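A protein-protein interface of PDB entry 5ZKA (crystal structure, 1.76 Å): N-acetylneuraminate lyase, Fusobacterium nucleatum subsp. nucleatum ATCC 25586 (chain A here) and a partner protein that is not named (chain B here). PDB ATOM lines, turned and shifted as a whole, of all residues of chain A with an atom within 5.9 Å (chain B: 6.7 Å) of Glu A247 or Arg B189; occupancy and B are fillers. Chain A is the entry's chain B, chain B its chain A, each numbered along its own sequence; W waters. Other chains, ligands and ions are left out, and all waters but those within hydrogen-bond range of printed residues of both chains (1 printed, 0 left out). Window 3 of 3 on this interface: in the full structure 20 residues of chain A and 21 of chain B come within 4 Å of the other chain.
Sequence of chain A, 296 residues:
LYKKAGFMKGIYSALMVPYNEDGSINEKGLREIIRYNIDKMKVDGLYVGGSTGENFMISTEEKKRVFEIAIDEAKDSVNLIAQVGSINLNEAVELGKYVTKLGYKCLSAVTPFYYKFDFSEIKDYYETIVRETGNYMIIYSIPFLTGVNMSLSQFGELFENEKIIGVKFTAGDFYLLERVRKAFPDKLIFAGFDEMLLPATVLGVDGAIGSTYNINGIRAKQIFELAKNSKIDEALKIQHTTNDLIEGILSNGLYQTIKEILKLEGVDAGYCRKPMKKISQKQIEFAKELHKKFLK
Printed residues of chain B within 4 Å of Asn A243: Tyr B185 (3.6 Å), Glu B188 (2.8 Å) and Arg B189 (3.4 Å).
Of the printed residues of chain B, Asp A244 touches Arg B189 and Lys B192.
Of the printed residues of chain B, Glu A247 touches Tyr B185 and Arg B189.
Of the printed residues of chain A, Glu B188 touches His A240 (2.6 Å) and Asn A243 (2.8 Å).
Arg B189 touches four residues of chain A.
Of the printed residues of chain A, Lys B192 touches His A240 and Asp A244.
The nearest residue of chain B that does not touch Glu A247 is Leu B162 (4.2 Å).
The nearest residue of chain A that does not touch Arg B189 is Gln A239 (5.0 Å).
The nearest printed residue of chain B that does not touch Asn A243 is Phe B184 (5.8 Å).
OE1 of Glu B188 lies within hydrogen-bond range of ND2 of Asn A243 (2.8 Å).
The side-chain carboxylate of Glu B188 sits at hydrogen-bond distance from a ring nitrogen (ND1) of His A240, at 2.6 Å.
NH2 of Arg B189 lies within hydrogen-bond range of O of His A240 (3.2 Å).
NH1 of Arg B189 lies within salt-bridge range of OE1 of Glu A247 (3.1 Å).
The side-chain carboxylate of Asp A244 is in salt-bridge range of the side-chain amino group of Lys B192 (3.5 Å).
The guanidinium group (NH1) of Arg B189 lies within salt-bridge range of the side-chain carboxylate (OD1) of Asp A244, 2.8 Å away.
Water W1 bridges the side-chain amino group of Lys B192 (3.1 Å) and the side-chain hydroxyl of Thr A241 (3.2 Å).
Among the printed residues, pairs that only touch across the chains: Glu A247 with Tyr B185 (3.4 Å), Asn A243 with Arg B189 (3.4 Å), His A240 with Lys B192 (3.6 Å), Asn A243 with Tyr B185 (3.6 Å) and His A240 with Arg B191 (3.96 Å).
Of the 14 printed residues of chain A, 4 touch a printed residue of chain B.
Of the 12 printed residues of chain B, 5 touch a printed residue of chain A.
OD1 of Asn A243 sits at hydrogen-bond distance from NE2 of Gln A239 (2.8 Å).
OE1 of Glu B188 lies within salt-bridge range of NE of Arg B189, 2.8 Å away.
The backbone carbonyl oxygen (O) of Phe B194 sits at hydrogen-bond distance from the guanidinium group (NH2) of Arg B191 (2.9 Å).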
ATOM      1  N   GLN A 239     -10.520 -22.553 -16.251  1.00  0.00           N
ATOM      2  CA  GLN A 239      -9.605 -22.999 -17.290  1.00  0.00           C
ATOM      3  C   GLN A 239     -10.176 -24.195 -18.053  1.00  0.00           C
ATOM      4  O   GLN A 239     -10.007 -24.297 -19.277  1.00  0.00           O
ATOM      5  CB  GLN A 239      -8.242 -23.356 -16.701  1.00  0.00           C
ATOM      6  CG  GLN A 239      -7.243 -23.761 -17.789  1.00  0.00           C
ATOM      7  CD  GLN A 239      -6.620 -22.555 -18.488  1.00  0.00           C
ATOM      8  OE1 GLN A 239      -5.895 -21.771 -17.867  1.00  0.00           O
ATOM      9  NE2 GLN A 239      -6.891 -22.411 -19.783  1.00  0.00           N
ATOM     10  N   HIS A 240     -10.883 -25.094 -17.359  1.00  0.00           N
ATOM     11  CA  HIS A 240     -11.552 -26.205 -18.049  1.00  0.00           C
ATOM     12  C   HIS A 240     -12.575 -25.690 -19.062  1.00  0.00           C
ATOM     13  O   HIS A 240     -12.608 -26.135 -20.216  1.00  0.00           O
ATOM     14  CB  HIS A 240     -12.262 -27.122 -17.044  1.00  0.00           C
ATOM     15  CG  HIS A 240     -11.371 -28.096 -16.334  1.00  0.00           C
ATOM     16  ND1 HIS A 240     -10.244 -28.647 -16.904  1.00  0.00           N
ATOM     17  CD2 HIS A 240     -11.476 -28.650 -15.100  1.00  0.00           C
ATOM     18  CE1 HIS A 240      -9.680 -29.481 -16.045  1.00  0.00           C
ATOM     19  NE2 HIS A 240     -10.410 -29.503 -14.944  1.00  0.00           N
ATOM     20  N   THR A 241     -13.456 -24.785 -18.631  1.00  0.00           N
ATOM     21  CA  THR A 241     -14.442 -24.207 -19.545  1.00  0.00           C
ATOM     22  C   THR A 241     -13.758 -23.486 -20.696  1.00  0.00           C
ATOM     23  O   THR A 241     -14.137 -23.655 -21.865  1.00  0.00           O
ATOM     24  CB  THR A 241     -15.367 -23.242 -18.797  1.00  0.00           C
ATOM     25  OG1 THR A 241     -15.978 -23.912 -17.692  1.00  0.00           O
ATOM     26  CG2 THR A 241     -16.464 -22.716 -19.730  1.00  0.00           C
ATOM     27  N   THR A 242     -12.767 -22.648 -20.373  1.00  0.00           N
ATOM     28  CA  THR A 242     -11.984 -21.947 -21.392  1.00  0.00           C
ATOM     29  C   THR A 242     -11.387 -22.911 -22.408  1.00  0.00           C
ATOM     30  O   THR A 242     -11.388 -22.634 -23.616  1.00  0.00           O
ATOM     31  CB  THR A 242     -10.885 -21.126 -20.705  1.00  0.00           C
ATOM     32  OG1 THR A 242     -11.489 -19.999 -20.069  1.00  0.00           O
ATOM     33  CG2 THR A 242      -9.829 -20.638 -21.696  1.00  0.00           C
ATOM     34  N   ASN A 243     -10.882 -24.057 -21.948  1.00  0.00           N
ATOM     35  CA  ASN A 243     -10.222 -24.958 -22.884  1.00  0.00           C
ATOM     36  C   ASN A 243     -11.209 -25.795 -23.702  1.00  0.00           C
ATOM     37  O   ASN A 243     -10.859 -26.223 -24.805  1.00  0.00           O
ATOM     38  CB  ASN A 243      -9.213 -25.834 -22.129  1.00  0.00           C
ATOM     39  CG  ASN A 243      -7.931 -25.076 -21.821  1.00  0.00           C
ATOM     40  OD1 ASN A 243      -7.883 -23.843 -21.942  1.00  0.00           O
ATOM     41  ND2 ASN A 243      -6.883 -25.798 -21.425  1.00  0.00           N
ATOM     42  N   ASP A 244     -12.439 -26.012 -23.219  1.00  0.00           N
ATOM     43  CA  ASP A 244     -13.497 -26.501 -24.108  1.00  0.00           C
ATOM     44  C   ASP A 244     -13.705 -25.548 -25.280  1.00  0.00           C
ATOM     45  O   ASP A 244     -13.832 -25.971 -26.438  1.00  0.00           O
ATOM     46  CB  ASP A 244     -14.807 -26.657 -23.341  1.00  0.00           C
ATOM     47  CG  ASP A 244     -14.799 -27.843 -22.384  1.00  0.00           C
ATOM     48  OD1 ASP A 244     -13.872 -28.687 -22.448  1.00  0.00           O
ATOM     49  OD2 ASP A 244     -15.745 -27.926 -21.572  1.00  0.00           O
ATOM     50  N   LEU A 245     -13.762 -24.246 -24.993  1.00  0.00           N
ATOM     51  CA  LEU A 245     -13.926 -23.264 -26.061  1.00  0.00           C
ATOM     52  C   LEU A 245     -12.721 -23.263 -26.990  1.00  0.00           C
ATOM     53  O   LEU A 245     -12.869 -23.255 -28.216  1.00  0.00           O
ATOM     54  CB  LEU A 245     -14.134 -21.870 -25.457  1.00  0.00           C
ATOM     55  CG  LEU A 245     -14.021 -20.664 -26.398  1.00  0.00           C
ATOM     56  CD1 LEU A 245     -15.086 -20.715 -27.499  1.00  0.00           C
ATOM     57  CD2 LEU A 245     -14.147 -19.374 -25.564  1.00  0.00           C
ATOM     58  N   ILE A 246     -11.509 -23.242 -26.419  1.00  0.00           N
ATOM     59  CA  ILE A 246     -10.301 -23.179 -27.241  1.00  0.00           C
ATOM     60  C   ILE A 246     -10.165 -24.431 -28.097  1.00  0.00           C
ATOM     61  O   ILE A 246      -9.770 -24.360 -29.270  1.00  0.00           O
ATOM     62  CB  ILE A 246      -9.066 -22.953 -26.345  1.00  0.00           C
ATOM     63  CG1 ILE A 246      -9.038 -21.500 -25.863  1.00  0.00           C
ATOM     64  CG2 ILE A 246      -7.789 -23.266 -27.109  1.00  0.00           C
ATOM     65  CD1 ILE A 246      -7.914 -21.186 -24.852  1.00  0.00           C
ATOM     66  N   GLU A 247     -10.469 -25.598 -27.528  1.00  0.00           N
ATOM     67  CA  GLU A 247     -10.438 -26.826 -28.313  1.00  0.00           C
ATOM     68  C   GLU A 247     -11.306 -26.698 -29.555  1.00  0.00           C
ATOM     69  O   GLU A 247     -10.894 -27.083 -30.656  1.00  0.00           O
ATOM     70  CB  GLU A 247     -10.910 -27.996 -27.456  1.00  0.00           C
ATOM     71  CG  GLU A 247     -10.968 -29.313 -28.195  1.00  0.00           C
ATOM     72  CD  GLU A 247     -11.629 -30.377 -27.352  1.00  0.00           C
ATOM     73  OE1 GLU A 247     -10.986 -30.853 -26.408  1.00  0.00           O
ATOM     74  OE2 GLU A 247     -12.799 -30.723 -27.613  1.00  0.00           O
ATOM     75  N   GLY A 248     -12.505 -26.137 -29.398  1.00  0.00           N
ATOM     76  CA  GLY A 248     -13.379 -25.951 -30.546  1.00  0.00           C
ATOM     77  C   GLY A 248     -12.871 -24.880 -31.491  1.00  0.00           C
ATOM     78  O   GLY A 248     -12.957 -25.026 -32.711  1.00  0.00           O
ATOM     79  N   ILE A 249     -12.344 -23.782 -30.945  1.00  0.00           N
ATOM     80  CA  ILE A 249     -11.778 -22.741 -31.797  1.00  0.00           C
ATOM     81  C   ILE A 249     -10.660 -23.321 -32.653  1.00  0.00           C
ATOM     82  O   ILE A 249     -10.598 -23.087 -33.868  1.00  0.00           O
ATOM     83  CB  ILE A 249     -11.284 -21.563 -30.933  1.00  0.00           C
ATOM     84  CG1 ILE A 249     -12.467 -20.789 -30.335  1.00  0.00           C
ATOM     85  CG2 ILE A 249     -10.370 -20.658 -31.731  1.00  0.00           C
ATOM     86  CD1 ILE A 249     -12.042 -19.703 -29.360  1.00  0.00           C
ATOM     87  N   LEU A 250      -9.782 -24.125 -32.040  1.00  0.00           N
ATOM     88  CA  LEU A 250      -8.652 -24.691 -32.773  1.00  0.00           C
ATOM     89  C   LEU A 250      -9.101 -25.654 -33.863  1.00  0.00           C
ATOM     90  O   LEU A 250      -8.544 -25.644 -34.962  1.00  0.00           O
ATOM     91  CB  LEU A 250      -7.694 -25.404 -31.819  1.00  0.00           C
ATOM     92  CG  LEU A 250      -6.897 -24.435 -30.943  1.00  0.00           C
ATOM     93  CD1 LEU A 250      -6.127 -25.215 -29.873  1.00  0.00           C
ATOM     94  CD2 LEU A 250      -5.954 -23.628 -31.820  1.00  0.00           C
ATOM     95  N   SER A 251     -10.068 -26.523 -33.575  1.00  0.00           N
ATOM     96  CA  SER A 251     -10.488 -27.458 -34.606  1.00  0.00           C
ATOM     97  C   SER A 251     -11.272 -26.768 -35.712  1.00  0.00           C
ATOM     98  O   SER A 251     -11.361 -27.311 -36.817  1.00  0.00           O
ATOM     99  CB  SER A 251     -11.324 -28.587 -34.004  1.00  0.00           C
ATOM    100  OG  SER A 251     -12.607 -28.136 -33.624  1.00  0.00           O
ATOM    101  N   ASN A 252     -11.831 -25.586 -35.448  1.00  0.00           N
ATOM    102  CA  ASN A 252     -12.629 -24.864 -36.441  1.00  0.00           C
ATOM    103  C   ASN A 252     -11.825 -23.830 -37.224  1.00  0.00           C
ATOM    104  O   ASN A 252     -12.363 -23.227 -38.161  1.00  0.00           O
ATOM    105  CB  ASN A 252     -13.827 -24.183 -35.764  1.00  0.00           C
ATOM    106  CG  ASN A 252     -14.984 -23.929 -36.723  1.00  0.00           C
ATOM    107  OD1 ASN A 252     -15.481 -24.849 -37.370  1.00  0.00           O
ATOM    108  ND2 ASN A 252     -15.442 -22.677 -36.786  1.00  0.00           N
ATOM    109  N   LEU B 162      -5.960 -37.666 -27.125  1.00  0.00           N
ATOM    110  CA  LEU B 162      -7.025 -37.634 -26.127  1.00  0.00           C
ATOM    111  C   LEU B 162      -8.071 -38.713 -26.388  1.00  0.00           C
ATOM    112  O   LEU B 162      -8.521 -39.387 -25.453  1.00  0.00           O
ATOM    113  CB  LEU B 162      -7.666 -36.247 -26.089  1.00  0.00           C
ATOM    114  CG  LEU B 162      -8.793 -35.991 -25.090  1.00  0.00           C
ATOM    115  CD1 LEU B 162      -8.320 -36.179 -23.651  1.00  0.00           C
ATOM    116  CD2 LEU B 162      -9.330 -34.581 -25.314  1.00  0.00           C
ATOM    117  N   PHE B 184       1.102 -29.567 -21.114  1.00  0.00           N
ATOM    118  CA  PHE B 184       0.125 -29.239 -20.083  1.00  0.00           C
ATOM    119  C   PHE B 184      -1.242 -28.871 -20.644  1.00  0.00           C
ATOM    120  O   PHE B 184      -2.211 -28.812 -19.883  1.00  0.00           O
ATOM    121  CB  PHE B 184       0.672 -28.113 -19.178  1.00  0.00           C
ATOM    122  CG  PHE B 184       1.689 -28.596 -18.192  1.00  0.00           C
ATOM    123  CD1 PHE B 184       2.958 -28.961 -18.609  1.00  0.00           C
ATOM    124  CD2 PHE B 184       1.373 -28.707 -16.850  1.00  0.00           C
ATOM    125  CE1 PHE B 184       3.898 -29.439 -17.697  1.00  0.00           C
ATOM    126  CE2 PHE B 184       2.306 -29.182 -15.933  1.00  0.00           C
ATOM    127  CZ  PHE B 184       3.564 -29.549 -16.358  1.00  0.00           C
ATOM    128  N   TYR B 185      -1.372 -28.661 -21.956  1.00  0.00           N
ATOM    129  CA  TYR B 185      -2.707 -28.599 -22.531  1.00  0.00           C
ATOM    130  C   TYR B 185      -3.340 -29.987 -22.540  1.00  0.00           C
ATOM    131  O   TYR B 185      -4.470 -30.183 -22.068  1.00  0.00           O
ATOM    132  CB  TYR B 185      -2.631 -28.010 -23.945  1.00  0.00           C
ATOM    133  CG  TYR B 185      -3.947 -27.965 -24.697  1.00  0.00           C
ATOM    134  CD1 TYR B 185      -5.130 -27.572 -24.074  1.00  0.00           C
ATOM    135  CD2 TYR B 185      -3.997 -28.299 -26.039  1.00  0.00           C
ATOM    136  CE1 TYR B 185      -6.342 -27.524 -24.780  1.00  0.00           C
ATOM    137  CE2 TYR B 185      -5.201 -28.253 -26.762  1.00  0.00           C
ATOM    138  CZ  TYR B 185      -6.367 -27.862 -26.126  1.00  0.00           C
ATOM    139  OH  TYR B 185      -7.551 -27.827 -26.842  1.00  0.00           O
ATOM    140  N   LEU B 186      -2.607 -30.979 -23.045  1.00  0.00           N
ATOM    141  CA  LEU B 186      -3.119 -32.346 -23.012  1.00  0.00           C
ATOM    142  C   LEU B 186      -3.395 -32.794 -21.577  1.00  0.00           C
ATOM    143  O   LEU B 186      -4.388 -33.488 -21.320  1.00  0.00           O
ATOM    144  CB  LEU B 186      -2.131 -33.288 -23.699  1.00  0.00           C
ATOM    145  CG  LEU B 186      -2.505 -34.771 -23.726  1.00  0.00           C
ATOM    146  CD1 LEU B 186      -3.727 -35.009 -24.604  1.00  0.00           C
ATOM    147  CD2 LEU B 186      -1.313 -35.591 -24.210  1.00  0.00           C
ATOM    148  N   LEU B 187      -2.539 -32.391 -20.621  1.00  0.00           N
ATOM    149  CA  LEU B 187      -2.765 -32.778 -19.229  1.00  0.00           C
ATOM    150  C   LEU B 187      -4.099 -32.244 -18.731  1.00  0.00           C
ATOM    151  O   LEU B 187      -4.871 -32.970 -18.100  1.00  0.00           O
ATOM    152  CB  LEU B 187      -1.616 -32.287 -18.338  1.00  0.00           C
ATOM    153  CG  LEU B 187      -1.766 -32.539 -16.826  1.00  0.00           C
ATOM    154  CD1 LEU B 187      -2.022 -34.023 -16.518  1.00  0.00           C
ATOM    155  CD2 LEU B 187      -0.560 -32.003 -16.038  1.00  0.00           C
ATOM    156  N   GLU B 188      -4.403 -30.979 -19.032  1.00  0.00           N
ATOM    157  CA  GLU B 188      -5.685 -30.418 -18.624  1.00  0.00           C
ATOM    158  C   GLU B 188      -6.851 -31.101 -19.338  1.00  0.00           C
ATOM    159  O   GLU B 188      -7.915 -31.305 -18.742  1.00  0.00           O
ATOM    160  CB  GLU B 188      -5.681 -28.901 -18.882  1.00  0.00           C
ATOM    161  CG  GLU B 188      -7.003 -28.180 -18.563  1.00  0.00           C
ATOM    162  CD  GLU B 188      -8.060 -28.354 -19.657  1.00  0.00           C
ATOM    163  OE1 GLU B 188      -7.671 -28.424 -20.842  1.00  0.00           O
ATOM    164  OE2 GLU B 188      -9.262 -28.438 -19.329  1.00  0.00           O
ATOM    165  N   ARG B 189      -6.684 -31.450 -20.622  1.00  0.00           N
ATOM    166  CA  ARG B 189      -7.773 -32.094 -21.364  1.00  0.00           C
ATOM    167  C   ARG B 189      -8.061 -33.493 -20.828  1.00  0.00           C
ATOM    168  O   ARG B 189      -9.224 -33.895 -20.729  1.00  0.00           O
ATOM    169  CB  ARG B 189      -7.435 -32.169 -22.858  1.00  0.00           C
ATOM    170  CG  ARG B 189      -7.407 -30.824 -23.598  1.00  0.00           C
ATOM    171  CD  ARG B 189      -8.817 -30.329 -23.914  1.00  0.00           C
ATOM    172  NE  ARG B 189      -9.382 -29.592 -22.788  1.00  0.00           N
ATOM    173  CZ  ARG B 189     -10.669 -29.298 -22.670  1.00  0.00           C
ATOM    174  NH1 ARG B 189     -11.529 -29.673 -23.609  1.00  0.00           N
ATOM    175  NH2 ARG B 189     -11.103 -28.640 -21.607  1.00  0.00           N
ATOM    176  N   VAL B 190      -7.014 -34.245 -20.478  1.00  0.00           N
ATOM    177  CA  VAL B 190      -7.208 -35.574 -19.891  1.00  0.00           C
ATOM    178  C   VAL B 190      -7.882 -35.456 -18.528  1.00  0.00           C
ATOM    179  O   VAL B 190      -8.801 -36.216 -18.213  1.00  0.00           O
ATOM    180  CB  VAL B 190      -5.857 -36.307 -19.797  1.00  0.00           C
ATOM    181  CG1 VAL B 190      -6.011 -37.619 -19.024  1.00  0.00           C
ATOM    182  CG2 VAL B 190      -5.315 -36.575 -21.208  1.00  0.00           C
ATOM    183  N   ARG B 191      -7.450 -34.480 -17.713  1.00  0.00           N
ATOM    184  CA  ARG B 191      -8.072 -34.269 -16.406  1.00  0.00           C
ATOM    185  C   ARG B 191      -9.555 -33.965 -16.540  1.00  0.00           C
ATOM    186  O   ARG B 191     -10.377 -34.492 -15.781  1.00  0.00           O
ATOM    187  CB  ARG B 191      -7.368 -33.131 -15.650  1.00  0.00           C
ATOM    188  CG  ARG B 191      -8.078 -32.689 -14.360  1.00  0.00           C
ATOM    189  CD  ARG B 191      -7.862 -33.657 -13.182  1.00  0.00           C
ATOM    190  NE  ARG B 191      -8.466 -34.972 -13.431  1.00  0.00           N
ATOM    191  CZ  ARG B 191      -8.117 -36.085 -12.798  1.00  0.00           C
ATOM    192  NH1 ARG B 191      -7.175 -36.043 -11.859  1.00  0.00           N
ATOM    193  NH2 ARG B 191      -8.702 -37.245 -13.118  1.00  0.00           N
ATOM    194  N   LYS B 192      -9.921 -33.114 -17.506  1.00  0.00           N
ATOM    195  CA  LYS B 192     -11.330 -32.766 -17.669  1.00  0.00           C
ATOM    196  C   LYS B 192     -12.138 -33.926 -18.227  1.00  0.00           C
ATOM    197  O   LYS B 192     -13.276 -34.149 -17.808  1.00  0.00           O
ATOM    198  CB  LYS B 192     -11.489 -31.548 -18.579  1.00  0.00           C
ATOM    199  CG  LYS B 192     -12.925 -31.007 -18.573  1.00  0.00           C
ATOM    200  CD  LYS B 192     -13.405 -30.614 -19.948  1.00  0.00           C
ATOM    201  CE  LYS B 192     -14.928 -30.632 -20.020  1.00  0.00           C
ATOM    202  NZ  LYS B 192     -15.567 -30.034 -18.818  1.00  0.00           N
ATOM    203  N   ALA B 193     -11.574 -34.669 -19.179  1.00  0.00           N
ATOM    204  CA  ALA B 193     -12.340 -35.715 -19.846  1.00  0.00           C
ATOM    205  C   ALA B 193     -12.554 -36.946 -18.973  1.00  0.00           C
ATOM    206  O   ALA B 193     -13.520 -37.688 -19.190  1.00  0.00           O
ATOM    207  CB  ALA B 193     -11.637 -36.131 -21.137  1.00  0.00           C
ATOM    208  N   PHE B 194     -11.667 -37.199 -18.015  1.00  0.00           N
ATOM    209  CA  PHE B 194     -11.685 -38.427 -17.216  1.00  0.00           C
ATOM    210  C   PHE B 194     -11.568 -38.072 -15.736  1.00  0.00           C
ATOM    211  O   PHE B 194     -10.557 -38.370 -15.091  1.00  0.00           O
ATOM    212  CB  PHE B 194     -10.558 -39.361 -17.659  1.00  0.00           C
ATOM    213  CG  PHE B 194     -10.454 -39.500 -19.160  1.00  0.00           C
ATOM    214  CD1 PHE B 194     -11.437 -40.178 -19.878  1.00  0.00           C
ATOM    215  CD2 PHE B 194      -9.391 -38.946 -19.849  1.00  0.00           C
ATOM    216  CE1 PHE B 194     -11.358 -40.294 -21.261  1.00  0.00           C
ATOM    217  CE2 PHE B 194      -9.306 -39.054 -21.230  1.00  0.00           C
ATOM    218  CZ  PHE B 194     -10.287 -39.726 -21.934  1.00  0.00           C
HETATM  219  O   HOH W   1     -16.273 -27.117 -17.999  1.00  0.00           O
